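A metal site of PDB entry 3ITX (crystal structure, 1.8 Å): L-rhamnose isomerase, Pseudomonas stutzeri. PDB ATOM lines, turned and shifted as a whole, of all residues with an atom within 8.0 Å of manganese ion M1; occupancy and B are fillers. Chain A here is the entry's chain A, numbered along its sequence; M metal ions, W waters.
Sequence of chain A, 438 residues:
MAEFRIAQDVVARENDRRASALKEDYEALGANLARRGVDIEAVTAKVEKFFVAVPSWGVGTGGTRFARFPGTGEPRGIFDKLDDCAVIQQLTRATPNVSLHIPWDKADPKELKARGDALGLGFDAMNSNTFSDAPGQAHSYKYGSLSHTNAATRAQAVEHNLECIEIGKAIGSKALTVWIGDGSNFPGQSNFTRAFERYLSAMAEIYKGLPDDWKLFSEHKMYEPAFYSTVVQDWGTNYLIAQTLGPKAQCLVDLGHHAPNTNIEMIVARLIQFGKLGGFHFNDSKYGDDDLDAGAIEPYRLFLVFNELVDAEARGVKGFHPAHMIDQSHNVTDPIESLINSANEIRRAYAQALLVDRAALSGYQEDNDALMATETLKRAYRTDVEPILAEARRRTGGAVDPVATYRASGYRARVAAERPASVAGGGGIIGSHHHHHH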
ATOM      1  N   TRP A  57      31.604 -36.546 -29.552  1.00  0.00           N
ATOM      2  CA  TRP A  57      32.304 -36.060 -30.741  1.00  0.00           C
ATOM      3  C   TRP A  57      33.454 -35.111 -30.417  1.00  0.00           C
ATOM      4  O   TRP A  57      34.152 -34.636 -31.313  1.00  0.00           O
ATOM      5  CB  TRP A  57      31.297 -35.381 -31.677  1.00  0.00           C
ATOM      6  CG  TRP A  57      30.626 -34.145 -31.112  1.00  0.00           C
ATOM      7  CD1 TRP A  57      31.065 -32.855 -31.232  1.00  0.00           C
ATOM      8  CD2 TRP A  57      29.421 -34.100 -30.343  1.00  0.00           C
ATOM      9  NE1 TRP A  57      30.192 -32.010 -30.587  1.00  0.00           N
ATOM     10  CE2 TRP A  57      29.178 -32.746 -30.032  1.00  0.00           C
ATOM     11  CE3 TRP A  57      28.521 -35.068 -29.883  1.00  0.00           C
ATOM     12  CZ2 TRP A  57      28.065 -32.330 -29.284  1.00  0.00           C
ATOM     13  CZ3 TRP A  57      27.417 -34.663 -29.137  1.00  0.00           C
ATOM     14  CH2 TRP A  57      27.198 -33.302 -28.853  1.00  0.00           C
ATOM     15  N   ASN A 127      21.607 -36.216 -29.676  1.00  0.00           N
ATOM     16  CA  ASN A 127      21.800 -35.189 -30.700  1.00  0.00           C
ATOM     17  C   ASN A 127      21.542 -35.805 -32.075  1.00  0.00           C
ATOM     18  O   ASN A 127      22.193 -36.786 -32.439  1.00  0.00           O
ATOM     19  CB  ASN A 127      23.222 -34.615 -30.648  1.00  0.00           C
ATOM     20  CG  ASN A 127      23.465 -33.812 -29.388  1.00  0.00           C
ATOM     21  OD1 ASN A 127      23.230 -32.606 -29.351  1.00  0.00           O
ATOM     22  ND2 ASN A 127      23.945 -34.490 -28.341  1.00  0.00           N
ATOM     23  N   THR A 177      18.352 -32.925 -28.627  1.00  0.00           N
ATOM     24  CA  THR A 177      18.792 -31.605 -29.052  1.00  0.00           C
ATOM     25  C   THR A 177      18.797 -31.589 -30.569  1.00  0.00           C
ATOM     26  O   THR A 177      19.361 -32.470 -31.210  1.00  0.00           O
ATOM     27  CB  THR A 177      20.201 -31.286 -28.538  1.00  0.00           C
ATOM     28  OG1 THR A 177      20.154 -31.084 -27.131  1.00  0.00           O
ATOM     29  CG2 THR A 177      20.758 -30.028 -29.205  1.00  0.00           C
ATOM     30  N   TRP A 179      19.885 -29.424 -33.791  1.00  0.00           N
ATOM     31  CA  TRP A 179      20.601 -28.335 -34.431  1.00  0.00           C
ATOM     32  C   TRP A 179      20.723 -28.745 -35.893  1.00  0.00           C
ATOM     33  O   TRP A 179      21.204 -29.836 -36.186  1.00  0.00           O
ATOM     34  CB  TRP A 179      22.019 -28.126 -33.896  1.00  0.00           C
ATOM     35  CG  TRP A 179      22.749 -27.105 -34.758  1.00  0.00           C
ATOM     36  CD1 TRP A 179      22.494 -25.758 -34.816  1.00  0.00           C
ATOM     37  CD2 TRP A 179      23.722 -27.375 -35.774  1.00  0.00           C
ATOM     38  NE1 TRP A 179      23.239 -25.176 -35.813  1.00  0.00           N
ATOM     39  CE2 TRP A 179      24.009 -26.142 -36.418  1.00  0.00           C
ATOM     40  CE3 TRP A 179      24.383 -28.530 -36.208  1.00  0.00           C
ATOM     41  CZ2 TRP A 179      24.919 -26.038 -37.471  1.00  0.00           C
ATOM     42  CZ3 TRP A 179      25.293 -28.426 -37.260  1.00  0.00           C
ATOM     43  CH2 TRP A 179      25.554 -27.184 -37.874  1.00  0.00           C
ATOM     44  N   GLU A 219      18.410 -25.527 -31.090  1.00  0.00           N
ATOM     45  CA  GLU A 219      19.607 -24.707 -30.964  1.00  0.00           C
ATOM     46  C   GLU A 219      19.776 -23.708 -32.101  1.00  0.00           C
ATOM     47  O   GLU A 219      19.909 -24.098 -33.263  1.00  0.00           O
ATOM     48  CB  GLU A 219      20.824 -25.627 -30.894  1.00  0.00           C
ATOM     49  CG  GLU A 219      22.152 -24.944 -30.649  1.00  0.00           C
ATOM     50  CD  GLU A 219      23.307 -25.936 -30.629  1.00  0.00           C
ATOM     51  OE1 GLU A 219      23.054 -27.152 -30.665  1.00  0.00           O
ATOM     52  OE2 GLU A 219      24.475 -25.482 -30.574  1.00  0.00           O
ATOM     53  N   HIS A 220      19.786 -22.413 -31.778  1.00  0.00           N
ATOM     54  CA  HIS A 220      19.939 -21.400 -32.805  1.00  0.00           C
ATOM     55  C   HIS A 220      21.404 -21.164 -33.150  1.00  0.00           C
ATOM     56  O   HIS A 220      22.296 -21.465 -32.358  1.00  0.00           O
ATOM     57  CB  HIS A 220      19.301 -20.066 -32.372  1.00  0.00           C
ATOM     58  CG  HIS A 220      19.869 -19.504 -31.106  1.00  0.00           C
ATOM     59  ND1 HIS A 220      19.382 -19.847 -29.865  1.00  0.00           N
ATOM     60  CD2 HIS A 220      20.857 -18.607 -30.887  1.00  0.00           C
ATOM     61  CE1 HIS A 220      20.052 -19.184 -28.932  1.00  0.00           C
ATOM     62  NE2 HIS A 220      20.956 -18.430 -29.534  1.00  0.00           N
ATOM     63  N   LYS A 221      21.637 -20.633 -34.341  1.00  0.00           N
ATOM     64  CA  LYS A 221      22.990 -20.346 -34.814  1.00  0.00           C
ATOM     65  C   LYS A 221      22.880 -19.300 -35.909  1.00  0.00           C
ATOM     66  O   LYS A 221      22.125 -19.467 -36.877  1.00  0.00           O
ATOM     67  CB  LYS A 221      23.639 -21.623 -35.358  1.00  0.00           C
ATOM     68  CG  LYS A 221      25.123 -21.467 -35.589  1.00  0.00           C
ATOM     69  CD  LYS A 221      25.767 -22.739 -36.125  1.00  0.00           C
ATOM     70  CE  LYS A 221      27.276 -22.551 -36.270  1.00  0.00           C
ATOM     71  NZ  LYS A 221      27.960 -23.762 -36.801  1.00  0.00           N
ATOM     72  N   LEU A 252      18.171 -23.954 -26.566  1.00  0.00           N
ATOM     73  CA  LEU A 252      19.536 -24.259 -26.167  1.00  0.00           C
ATOM     74  C   LEU A 252      20.419 -23.107 -26.642  1.00  0.00           C
ATOM     75  O   LEU A 252      20.397 -22.728 -27.815  1.00  0.00           O
ATOM     76  CB  LEU A 252      19.969 -25.595 -26.768  1.00  0.00           C
ATOM     77  CG  LEU A 252      21.318 -26.150 -26.302  1.00  0.00           C
ATOM     78  CD1 LEU A 252      21.289 -27.675 -26.331  1.00  0.00           C
ATOM     79  CD2 LEU A 252      22.421 -25.613 -27.196  1.00  0.00           C
ATOM     80  N   VAL A 253      21.187 -22.547 -25.713  1.00  0.00           N
ATOM     81  CA  VAL A 253      22.077 -21.438 -26.023  1.00  0.00           C
ATOM     82  C   VAL A 253      23.527 -21.908 -26.108  1.00  0.00           C
ATOM     83  O   VAL A 253      24.092 -22.372 -25.120  1.00  0.00           O
ATOM     84  CB  VAL A 253      21.974 -20.337 -24.924  1.00  0.00           C
ATOM     85  CG1 VAL A 253      22.876 -19.158 -25.250  1.00  0.00           C
ATOM     86  CG2 VAL A 253      20.524 -19.874 -24.797  1.00  0.00           C
ATOM     87  N   ASP A 254      24.102 -21.826 -27.305  1.00  0.00           N
ATOM     88  CA  ASP A 254      25.496 -22.215 -27.527  1.00  0.00           C
ATOM     89  C   ASP A 254      26.262 -20.890 -27.602  1.00  0.00           C
ATOM     90  O   ASP A 254      26.052 -20.093 -28.515  1.00  0.00           O
ATOM     91  CB  ASP A 254      25.637 -22.981 -28.848  1.00  0.00           C
ATOM     92  CG  ASP A 254      27.046 -23.466 -29.088  1.00  0.00           C
ATOM     93  OD1 ASP A 254      27.979 -22.638 -29.056  1.00  0.00           O
ATOM     94  OD2 ASP A 254      27.224 -24.675 -29.321  1.00  0.00           O
ATOM     95  N   LEU A 255      27.153 -20.664 -26.635  1.00  0.00           N
ATOM     96  CA  LEU A 255      27.888 -19.415 -26.538  1.00  0.00           C
ATOM     97  C   LEU A 255      28.485 -18.831 -27.824  1.00  0.00           C
ATOM     98  O   LEU A 255      28.403 -17.618 -28.029  1.00  0.00           O
ATOM     99  CB  LEU A 255      28.979 -19.555 -25.461  1.00  0.00           C
ATOM    100  CG  LEU A 255      28.451 -20.030 -24.102  1.00  0.00           C
ATOM    101  CD1 LEU A 255      29.562 -19.929 -23.072  1.00  0.00           C
ATOM    102  CD2 LEU A 255      27.244 -19.197 -23.656  1.00  0.00           C
ATOM    103  N   GLY A 256      29.058 -19.663 -28.686  1.00  0.00           N
ATOM    104  CA  GLY A 256      29.654 -19.139 -29.905  1.00  0.00           C
ATOM    105  C   GLY A 256      28.710 -18.967 -31.090  1.00  0.00           C
ATOM    106  O   GLY A 256      29.167 -18.710 -32.203  1.00  0.00           O
ATOM    107  N   HIS A 257      27.402 -19.067 -30.861  1.00  0.00           N
ATOM    108  CA  HIS A 257      26.440 -18.954 -31.964  1.00  0.00           C
ATOM    109  C   HIS A 257      25.742 -17.614 -32.136  1.00  0.00           C
ATOM    110  O   HIS A 257      24.662 -17.553 -32.738  1.00  0.00           O
ATOM    111  CB  HIS A 257      25.359 -20.036 -31.816  1.00  0.00           C
ATOM    112  CG  HIS A 257      25.865 -21.420 -32.073  1.00  0.00           C
ATOM    113  ND1 HIS A 257      25.012 -22.489 -32.266  1.00  0.00           N
ATOM    114  CD2 HIS A 257      27.117 -21.915 -32.172  1.00  0.00           C
ATOM    115  CE1 HIS A 257      25.729 -23.583 -32.472  1.00  0.00           C
ATOM    116  NE2 HIS A 257      27.001 -23.257 -32.419  1.00  0.00           N
ATOM    117  N   PHE A 280      22.641 -25.155 -21.934  1.00  0.00           N
ATOM    118  CA  PHE A 280      23.780 -24.483 -22.536  1.00  0.00           C
ATOM    119  C   PHE A 280      24.742 -25.406 -23.254  1.00  0.00           C
ATOM    120  O   PHE A 280      24.875 -26.580 -22.925  1.00  0.00           O
ATOM    121  CB  PHE A 280      24.593 -23.752 -21.465  1.00  0.00           C
ATOM    122  CG  PHE A 280      23.872 -22.630 -20.822  1.00  0.00           C
ATOM    123  CD1 PHE A 280      23.932 -21.348 -21.358  1.00  0.00           C
ATOM    124  CD2 PHE A 280      23.124 -22.840 -19.673  1.00  0.00           C
ATOM    125  CE1 PHE A 280      23.258 -20.291 -20.755  1.00  0.00           C
ATOM    126  CE2 PHE A 280      22.442 -21.792 -19.058  1.00  0.00           C
ATOM    127  CZ  PHE A 280      22.506 -20.514 -19.602  1.00  0.00           C
ATOM    128  N   HIS A 281      25.426 -24.833 -24.231  1.00  0.00           N
ATOM    129  CA  HIS A 281      26.466 -25.528 -24.969  1.00  0.00           C
ATOM    130  C   HIS A 281      27.645 -24.623 -24.683  1.00  0.00           C
ATOM    131  O   HIS A 281      27.753 -23.539 -25.242  1.00  0.00           O
ATOM    132  CB  HIS A 281      26.175 -25.550 -26.474  1.00  0.00           C
ATOM    133  CG  HIS A 281      25.531 -26.818 -26.949  1.00  0.00           C
ATOM    134  ND1 HIS A 281      25.465 -27.167 -28.285  1.00  0.00           N
ATOM    135  CD2 HIS A 281      24.927 -27.829 -26.271  1.00  0.00           C
ATOM    136  CE1 HIS A 281      24.847 -28.331 -28.408  1.00  0.00           C
ATOM    137  NE2 HIS A 281      24.510 -28.755 -27.204  1.00  0.00           N
ATOM    138  N   PHE A 282      28.516 -25.065 -23.781  1.00  0.00           N
ATOM    139  CA  PHE A 282      29.677 -24.268 -23.400  1.00  0.00           C
ATOM    140  C   PHE A 282      30.861 -24.430 -24.336  1.00  0.00           C
ATOM    141  O   PHE A 282      31.142 -25.523 -24.819  1.00  0.00           O
ATOM    142  CB  PHE A 282      30.124 -24.614 -21.973  1.00  0.00           C
ATOM    143  CG  PHE A 282      29.141 -24.229 -20.920  1.00  0.00           C
ATOM    144  CD1 PHE A 282      28.244 -25.148 -20.407  1.00  0.00           C
ATOM    145  CD2 PHE A 282      29.090 -22.920 -20.450  1.00  0.00           C
ATOM    146  CE1 PHE A 282      27.305 -24.783 -19.444  1.00  0.00           C
ATOM    147  CE2 PHE A 282      28.155 -22.542 -19.492  1.00  0.00           C
ATOM    148  CZ  PHE A 282      27.254 -23.471 -18.989  1.00  0.00           C
ATOM    149  N   ASN A 283      31.536 -23.313 -24.560  1.00  0.00           N
ATOM    150  CA  ASN A 283      32.728 -23.216 -25.396  1.00  0.00           C
ATOM    151  C   ASN A 283      33.122 -21.756 -25.376  1.00  0.00           C
ATOM    152  O   ASN A 283      32.445 -20.936 -24.769  1.00  0.00           O
ATOM    153  CB  ASN A 283      32.440 -23.686 -26.836  1.00  0.00           C
ATOM    154  CG  ASN A 283      31.228 -22.996 -27.455  1.00  0.00           C
ATOM    155  OD1 ASN A 283      31.167 -21.764 -27.570  1.00  0.00           O
ATOM    156  ND2 ASN A 283      30.240 -23.792 -27.863  1.00  0.00           N
ATOM    157  N   ASP A 289      31.928 -19.184 -34.604  1.00  0.00           N
ATOM    158  CA  ASP A 289      31.615 -20.339 -33.787  1.00  0.00           C
ATOM    159  C   ASP A 289      32.924 -21.118 -33.710  1.00  0.00           C
ATOM    160  O   ASP A 289      33.051 -22.217 -34.253  1.00  0.00           O
ATOM    161  CB  ASP A 289      30.521 -21.177 -34.448  1.00  0.00           C
ATOM    162  CG  ASP A 289      30.104 -22.369 -33.610  1.00  0.00           C
ATOM    163  OD1 ASP A 289      30.137 -22.263 -32.372  1.00  0.00           O
ATOM    164  OD2 ASP A 289      29.732 -23.406 -34.196  1.00  0.00           O
ATOM    165  N   ASP A 291      34.371 -22.652 -31.308  1.00  0.00           N
ATOM    166  CA  ASP A 291      34.351 -23.889 -30.532  1.00  0.00           C
ATOM    167  C   ASP A 291      35.630 -24.154 -29.737  1.00  0.00           C
ATOM    168  O   ASP A 291      36.090 -25.298 -29.638  1.00  0.00           O
ATOM    169  CB  ASP A 291      34.064 -25.074 -31.448  1.00  0.00           C
ATOM    170  CG  ASP A 291      32.622 -25.091 -31.918  1.00  0.00           C
ATOM    171  OD1 ASP A 291      31.750 -24.866 -31.061  1.00  0.00           O
ATOM    172  OD2 ASP A 291      32.361 -25.341 -33.114  1.00  0.00           O
ATOM    173  N   MET A 325      26.031 -28.681 -21.161  1.00  0.00           N
ATOM    174  CA  MET A 325      26.859 -29.525 -22.009  1.00  0.00           C
ATOM    175  C   MET A 325      28.010 -28.740 -22.611  1.00  0.00           C
ATOM    176  O   MET A 325      27.906 -27.540 -22.847  1.00  0.00           O
ATOM    177  CB  MET A 325      26.030 -30.124 -23.155  1.00  0.00           C
ATOM    178  CG  MET A 325      24.696 -30.712 -22.734  1.00  0.00           C
ATOM    179  SD  MET A 325      23.341 -29.541 -22.972  1.00  0.00           S
ATOM    180  CE  MET A 325      22.107 -30.601 -23.729  1.00  0.00           C
ATOM    181  N   ILE A 326      29.127 -29.426 -22.842  1.00  0.00           N
ATOM    182  CA  ILE A 326      30.275 -28.806 -23.475  1.00  0.00           C
ATOM    183  C   ILE A 326      30.152 -29.168 -24.951  1.00  0.00           C
ATOM    184  O   ILE A 326      29.898 -30.321 -25.285  1.00  0.00           O
ATOM    185  CB  ILE A 326      31.608 -29.390 -22.928  1.00  0.00           C
ATOM    186  CG1 ILE A 326      31.827 -28.932 -21.484  1.00  0.00           C
ATOM    187  CG2 ILE A 326      32.775 -28.950 -23.812  1.00  0.00           C
ATOM    188  CD1 ILE A 326      33.031 -29.573 -20.819  1.00  0.00           C
ATOM    189  N   ASP A 327      30.295 -28.174 -25.823  1.00  0.00           N
ATOM    190  CA  ASP A 327      30.252 -28.419 -27.261  1.00  0.00           C
ATOM    191  C   ASP A 327      31.451 -27.688 -27.808  1.00  0.00           C
ATOM    192  O   ASP A 327      31.403 -26.479 -28.042  1.00  0.00           O
ATOM    193  CB  ASP A 327      28.965 -27.875 -27.887  1.00  0.00           C
ATOM    194  CG  ASP A 327      28.872 -28.190 -29.382  1.00  0.00           C
ATOM    195  OD1 ASP A 327      29.723 -28.959 -29.877  1.00  0.00           O
ATOM    196  OD2 ASP A 327      27.949 -27.687 -30.042  1.00  0.00           O
ATOM    197  N   GLN A 328      32.539 -28.425 -28.006  1.00  0.00           N
ATOM    198  CA  GLN A 328      33.783 -27.824 -28.498  1.00  0.00           C
ATOM    199  C   GLN A 328      34.465 -28.688 -29.545  1.00  0.00           C
ATOM    200  O   GLN A 328      34.102 -29.845 -29.751  1.00  0.00           O
ATOM    201  CB  GLN A 328      34.743 -27.616 -27.318  1.00  0.00           C
ATOM    202  CG  GLN A 328      34.217 -26.661 -26.252  1.00  0.00           C
ATOM    203  CD  GLN A 328      35.034 -26.649 -24.967  1.00  0.00           C
ATOM    204  OE1 GLN A 328      34.739 -25.882 -24.051  1.00  0.00           O
ATOM    205  NE2 GLN A 328      36.058 -27.490 -24.898  1.00  0.00           N
HETATM  206 MN    MN M   1      26.173 -26.522 -29.990  1.00  0.00          MN
HETATM  207 MN    MN M   2      28.272 -24.752 -33.137  1.00  0.00          MN
HETATM  208  O   HOH W   1      26.968 -26.430 -32.249  1.00  0.00           O
HETATM  209  O   HOH W   2      25.374 -28.298 -31.660  1.00  0.00           O
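O of His 281 sits at hydrogen-bond distance from N of Leu 255, 3.3 Å away. The side-chain amide nitrogen (ND2) of Asn 283 is in hydrogen-bond range of the backbone carbonyl oxygen (O) of Asp 327. The side-chain carboxylate (OE2) of Glu 219 lies close to a ring nitrogen (ND1) of His 257 (3.5 Å). The backbone NH (N) of His 281 lies within hydrogen-bond range of the backbone carbonyl oxygen (O) of Val 253 (2.9 Å). N of Asp 327 lies within hydrogen-bond range of O of Phe 282, at 3.0 Å. ND2 of Asn 283 lies within hydrogen-bond range of OD1 of Asp 254 (2.8 Å). A ring nitrogen (ND1) of His 257 is in hydrogen-bond range of the backbone carbonyl oxygen (O) of His 220, at 2.9 Å. N of Gly 256 sits at hydrogen-bond distance from OD1 of Asp 254 (3.2 Å).
Merely in contact with manganese ion M1: His 257 (3.9 Å). Of the 23 residues printed, 5 come within 4 Å of manganese ion M1. Along chain A the residues within 4 Å of manganese ion M1 span positions 219 to 327. The nearest printed residue that does not touch manganese ion M1 is Leu 252 (4.8 Å).
Manganese ion M1 is bound by a ring nitrogen (ND1) of His 281 (2.0 Å), the side-chain carboxylate (OE2) of Glu 219 (2.1 Å), the side-chain carboxylate (OD2) of Asp 327 (2.1 Å), the side-chain carboxylate (OD2) of Asp 254 (2.2 Å), water W1 (2.4 Å) and water W2 (2.6 Å).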
